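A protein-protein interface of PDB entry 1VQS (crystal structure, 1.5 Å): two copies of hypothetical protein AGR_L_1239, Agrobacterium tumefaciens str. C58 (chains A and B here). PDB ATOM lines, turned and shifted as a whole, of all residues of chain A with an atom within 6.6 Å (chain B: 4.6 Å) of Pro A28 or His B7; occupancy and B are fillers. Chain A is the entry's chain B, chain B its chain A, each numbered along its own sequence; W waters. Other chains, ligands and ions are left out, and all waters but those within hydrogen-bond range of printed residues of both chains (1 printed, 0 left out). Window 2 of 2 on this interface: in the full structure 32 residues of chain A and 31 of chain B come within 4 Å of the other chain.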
ATOM      1  N   LEU A  22       3.060 -26.947  12.423  1.00  0.00           N
ATOM      2  CA  LEU A  22       3.933 -28.089  12.520  1.00  0.00           C
ATOM      3  C   LEU A  22       3.196 -29.418  12.608  1.00  0.00           C
ATOM      4  O   LEU A  22       2.028 -29.497  12.976  1.00  0.00           O
ATOM      5  CB  LEU A  22       4.863 -27.994  13.750  1.00  0.00           C
ATOM      6  CG  LEU A  22       5.622 -26.683  13.946  1.00  0.00           C
ATOM      7  CD1 LEU A  22       6.665 -26.844  15.062  1.00  0.00           C
ATOM      8  CD2 LEU A  22       6.306 -26.241  12.679  1.00  0.00           C
ATOM      9  N   GLY A  25       2.802 -32.269  17.775  1.00  0.00           N
ATOM     10  CA  GLY A  25       3.718 -32.538  18.865  1.00  0.00           C
ATOM     11  C   GLY A  25       5.152 -32.135  18.613  1.00  0.00           C
ATOM     12  O   GLY A  25       6.019 -32.389  19.447  1.00  0.00           O
ATOM     13  N   ALA A  26       5.420 -31.523  17.461  1.00  0.00           N
ATOM     14  CA  ALA A  26       6.788 -31.191  17.069  1.00  0.00           C
ATOM     15  C   ALA A  26       7.360 -29.893  17.632  1.00  0.00           C
ATOM     16  O   ALA A  26       8.533 -29.612  17.407  1.00  0.00           O
ATOM     17  CB  ALA A  26       6.879 -31.152  15.568  1.00  0.00           C
ATOM     18  N   ILE A  27       6.562 -29.078  18.323  1.00  0.00           N
ATOM     19  CA  ILE A  27       7.074 -27.777  18.795  1.00  0.00           C
ATOM     20  C   ILE A  27       8.371 -27.890  19.611  1.00  0.00           C
ATOM     21  O   ILE A  27       9.345 -27.208  19.302  1.00  0.00           O
ATOM     22  CB  ILE A  27       6.009 -26.945  19.530  1.00  0.00           C
ATOM     23  CG1 ILE A  27       5.029 -26.308  18.532  1.00  0.00           C
ATOM     24  CG2 ILE A  27       6.660 -25.769  20.311  1.00  0.00           C
ATOM     25  CD1 ILE A  27       3.873 -25.555  19.198  1.00  0.00           C
ATOM     26  N   PRO A  28       8.409 -28.754  20.627  1.00  0.00           N
ATOM     27  CA  PRO A  28       9.663 -28.811  21.410  1.00  0.00           C
ATOM     28  C   PRO A  28      10.885 -29.197  20.572  1.00  0.00           C
ATOM     29  O   PRO A  28      11.940 -28.557  20.729  1.00  0.00           O
ATOM     30  CB  PRO A  28       9.371 -29.858  22.493  1.00  0.00           C
ATOM     31  CG  PRO A  28       7.863 -29.863  22.621  1.00  0.00           C
ATOM     32  CD  PRO A  28       7.360 -29.605  21.210  1.00  0.00           C
ATOM     33  N   ALA A  29      10.769 -30.194  19.700  1.00  0.00           N
ATOM     34  CA  ALA A  29      11.905 -30.557  18.829  1.00  0.00           C
ATOM     35  C   ALA A  29      12.333 -29.449  17.888  1.00  0.00           C
ATOM     36  O   ALA A  29      13.531 -29.199  17.674  1.00  0.00           O
ATOM     37  CB  ALA A  29      11.605 -31.825  18.049  1.00  0.00           C
ATOM     38  N   TYR A  30      11.340 -28.770  17.327  1.00  0.00           N
ATOM     39  CA  TYR A  30      11.569 -27.661  16.419  1.00  0.00           C
ATOM     40  C   TYR A  30      12.310 -26.532  17.119  1.00  0.00           C
ATOM     41  O   TYR A  30      13.321 -26.008  16.623  1.00  0.00           O
ATOM     42  CB  TYR A  30      10.221 -27.190  15.845  1.00  0.00           C
ATOM     43  CG  TYR A  30      10.296 -25.985  14.964  1.00  0.00           C
ATOM     44  CD1 TYR A  30      10.267 -24.705  15.515  1.00  0.00           C
ATOM     45  CD2 TYR A  30      10.322 -26.087  13.575  1.00  0.00           C
ATOM     46  CE1 TYR A  30      10.324 -23.579  14.711  1.00  0.00           C
ATOM     47  CE2 TYR A  30      10.385 -24.950  12.770  1.00  0.00           C
ATOM     48  CZ  TYR A  30      10.395 -23.702  13.346  1.00  0.00           C
ATOM     49  OH  TYR A  30      10.451 -22.568  12.558  1.00  0.00           O
ATOM     50  N   LEU A  31      11.798 -26.121  18.271  1.00  0.00           N
ATOM     51  CA  LEU A  31      12.413 -24.987  18.963  1.00  0.00           C
ATOM     52  C   LEU A  31      13.826 -25.305  19.416  1.00  0.00           C
ATOM     53  O   LEU A  31      14.700 -24.423  19.406  1.00  0.00           O
ATOM     54  CB  LEU A  31      11.573 -24.558  20.153  1.00  0.00           C
ATOM     55  CG  LEU A  31      10.240 -23.920  19.768  1.00  0.00           C
ATOM     56  CD1 LEU A  31       9.450 -23.689  21.050  1.00  0.00           C
ATOM     57  CD2 LEU A  31      10.427 -22.616  19.017  1.00  0.00           C
ATOM     58  N   LYS A  32      14.058 -26.560  19.793  1.00  0.00           N
ATOM     59  CA  LYS A  32      15.395 -26.961  20.230  1.00  0.00           C
ATOM     60  C   LYS A  32      16.409 -26.800  19.106  1.00  0.00           C
ATOM     61  O   LYS A  32      17.443 -26.169  19.276  1.00  0.00           O
ATOM     62  CB  LYS A  32      15.397 -28.388  20.759  1.00  0.00           C
ATOM     63  CG  LYS A  32      16.796 -28.867  21.170  1.00  0.00           C
ATOM     64  CD  LYS A  32      16.817 -30.357  21.507  1.00  0.00           C
ATOM     65  CE  LYS A  32      16.123 -30.667  22.834  1.00  0.00           C
ATOM     66  NZ  LYS A  32      16.978 -30.339  24.015  1.00  0.00           N
ATOM     67  N   VAL A  33      16.108 -27.383  17.952  1.00  0.00           N
ATOM     68  CA  VAL A  33      17.072 -27.383  16.858  1.00  0.00           C
ATOM     69  C   VAL A  33      17.208 -25.985  16.232  1.00  0.00           C
ATOM     70  O   VAL A  33      18.295 -25.583  15.831  1.00  0.00           O
ATOM     71  CB  VAL A  33      16.751 -28.489  15.822  1.00  0.00           C
ATOM     72  CG1 VAL A  33      15.597 -28.094  14.936  1.00  0.00           C
ATOM     73  CG2 VAL A  33      17.983 -28.818  14.981  1.00  0.00           C
ATOM     74  N   GLU A  35      16.951 -23.133  17.984  1.00  0.00           N
ATOM     75  CA  GLU A  35      17.842 -22.461  18.918  1.00  0.00           C
ATOM     76  C   GLU A  35      19.299 -22.868  18.718  1.00  0.00           C
ATOM     77  O   GLU A  35      20.184 -22.012  18.633  1.00  0.00           O
ATOM     78  CB  GLU A  35      17.457 -22.731  20.374  1.00  0.00           C
ATOM     79  CG  GLU A  35      18.425 -22.068  21.339  1.00  0.00           C
ATOM     80  CD  GLU A  35      17.934 -21.974  22.741  1.00  0.00           C
ATOM     81  OE1 GLU A  35      16.865 -22.488  23.040  1.00  0.00           O
ATOM     82  OE2 GLU A  35      18.654 -21.341  23.554  1.00  0.00           O
ATOM     83  N   PHE A  54       5.452 -19.413  19.806  1.00  0.00           N
ATOM     84  CA  PHE A  54       4.789 -20.699  19.628  1.00  0.00           C
ATOM     85  C   PHE A  54       3.439 -20.693  20.327  1.00  0.00           C
ATOM     86  O   PHE A  54       3.194 -19.912  21.233  1.00  0.00           O
ATOM     87  CB  PHE A  54       5.650 -21.876  20.104  1.00  0.00           C
ATOM     88  CG  PHE A  54       5.990 -21.858  21.546  1.00  0.00           C
ATOM     89  CD1 PHE A  54       7.071 -21.121  22.017  1.00  0.00           C
ATOM     90  CD2 PHE A  54       5.257 -22.608  22.445  1.00  0.00           C
ATOM     91  CE1 PHE A  54       7.394 -21.143  23.350  1.00  0.00           C
ATOM     92  CE2 PHE A  54       5.566 -22.622  23.787  1.00  0.00           C
ATOM     93  CZ  PHE A  54       6.629 -21.885  24.238  1.00  0.00           C
ATOM     94  N   HIS B   7      10.973 -25.341  26.782  1.00  0.00           N
ATOM     95  CA  HIS B   7      11.311 -24.566  25.540  1.00  0.00           C
ATOM     96  C   HIS B   7      10.903 -23.073  25.553  1.00  0.00           C
ATOM     97  O   HIS B   7      10.806 -22.468  24.510  1.00  0.00           O
ATOM     98  CB  HIS B   7      10.755 -25.280  24.290  1.00  0.00           C
ATOM     99  CG  HIS B   7       9.292 -25.588  24.356  1.00  0.00           C
ATOM    100  ND1 HIS B   7       8.809 -26.845  24.651  1.00  0.00           N
ATOM    101  CD2 HIS B   7       8.206 -24.807  24.152  1.00  0.00           C
ATOM    102  CE1 HIS B   7       7.486 -26.821  24.636  1.00  0.00           C
ATOM    103  NE2 HIS B   7       7.095 -25.598  24.331  1.00  0.00           N
ATOM    104  N   HIS B   8      10.670 -22.499  26.736  1.00  0.00           N
ATOM    105  CA  HIS B   8      10.531 -21.045  26.905  1.00  0.00           C
ATOM    106  C   HIS B   8      11.205 -20.677  28.225  1.00  0.00           C
ATOM    107  O   HIS B   8      11.408 -21.553  29.072  1.00  0.00           O
ATOM    108  CB  HIS B   8       9.060 -20.616  26.913  1.00  0.00           C
ATOM    109  CG  HIS B   8       8.280 -21.145  28.081  1.00  0.00           C
ATOM    110  ND1 HIS B   8       7.577 -22.330  28.035  1.00  0.00           N
ATOM    111  CD2 HIS B   8       8.106 -20.654  29.331  1.00  0.00           C
ATOM    112  CE1 HIS B   8       7.000 -22.543  29.206  1.00  0.00           C
ATOM    113  NE2 HIS B   8       7.305 -21.541  30.011  1.00  0.00           N
ATOM    114  N   PRO B 109       6.725 -16.707  23.902  1.00  0.00           N
ATOM    115  CA  PRO B 109       7.976 -16.460  23.211  1.00  0.00           C
ATOM    116  C   PRO B 109       8.942 -17.639  23.275  1.00  0.00           C
ATOM    117  O   PRO B 109       9.106 -18.257  24.335  1.00  0.00           O
ATOM    118  CB  PRO B 109       8.545 -15.262  23.964  1.00  0.00           C
ATOM    119  CG  PRO B 109       8.059 -15.447  25.351  1.00  0.00           C
ATOM    120  CD  PRO B 109       6.668 -15.998  25.190  1.00  0.00           C
ATOM    121  N   ALA B 110       9.558 -17.968  22.133  1.00  0.00           N
ATOM    122  CA  ALA B 110      10.717 -18.851  22.152  1.00  0.00           C
ATOM    123  C   ALA B 110      11.847 -18.239  22.979  1.00  0.00           C
ATOM    124  O   ALA B 110      11.896 -17.033  23.180  1.00  0.00           O
ATOM    125  CB  ALA B 110      11.200 -19.091  20.734  1.00  0.00           C
ATOM    126  N   ARG B 111      12.777 -19.073  23.437  1.00  0.00           N
ATOM    127  CA  ARG B 111      13.878 -18.579  24.263  1.00  0.00           C
ATOM    128  C   ARG B 111      14.728 -17.559  23.529  1.00  0.00           C
ATOM    129  O   ARG B 111      15.373 -16.706  24.156  1.00  0.00           O
ATOM    130  CB  ARG B 111      14.759 -19.743  24.695  1.00  0.00           C
ATOM    131  CG  ARG B 111      14.085 -20.627  25.710  1.00  0.00           C
ATOM    132  CD  ARG B 111      14.705 -22.020  25.859  1.00  0.00           C
ATOM    133  NE  ARG B 111      16.159 -21.978  25.803  1.00  0.00           N
ATOM    134  CZ  ARG B 111      16.955 -21.619  26.803  1.00  0.00           C
ATOM    135  NH1 ARG B 111      16.462 -21.269  27.988  1.00  0.00           N
ATOM    136  NH2 ARG B 111      18.270 -21.616  26.609  1.00  0.00           N
HETATM  137  O   HOH W   1      18.176 -18.474  23.373  1.00  0.00           O
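The side-chain carboxylate (OE1) of Glu A35 is in salt-bridge range of the guanidinium group (NE) of Arg B111 (2.9 Å).
Among the printed residues, merely in contact across the chains: Pro A28 with His B7 (3.7 Å), Leu A31 with His B7 (3.5 Å), Leu A31 with Ala B110 (3.996 Å), Phe A54 with His B7 (3.3 Å), Phe A54 with His B8 (3.8 Å) and Phe A54 with Pro B109 (3.5 Å).
Pro A28 touches one residue of chain B. His B7 touches just these residues of chain A: Pro A28 (3.7 Å), Leu A31 (3.5 Å) and Phe A54 (3.3 Å). Of the printed residues of chain B, Glu A35 touches Arg B111. Of the printed residues of chain A, Ala B110 touches Leu A31 (3.996 Å). Of the printed residues of chain A, Pro B109 touches Phe A54. Of the printed residues of chain A, His B8 touches Phe A54 (3.8 Å). Of the printed residues of chain B, Leu A31 touches His B7 and Ala B110. The nearest printed residue of chain B that does not touch Pro A28 is His B8 (8.3 Å). The nearest printed residue of chain B that does not touch Phe A54 is Ala B110 (4.02 Å).
Of the 12 printed residues of chain A, 4 touch a printed residue of chain B. Printed residues of chain A that touch a printed residue of chain B: Pro A28, Leu A31, Glu A35 and Phe A54. Hydrophobic or aromatic side chains of chain A that line the printed part of chain B: Pro A28, Leu A31 and Phe A54.
No position is printed for both chains.
Water W1 lies within hydrogen-bond range of the side-chain carboxylate (OE2) of Glu A35 (2.9 Å) and the backbone carbonyl oxygen (O) of Arg B111 (3.4 Å).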
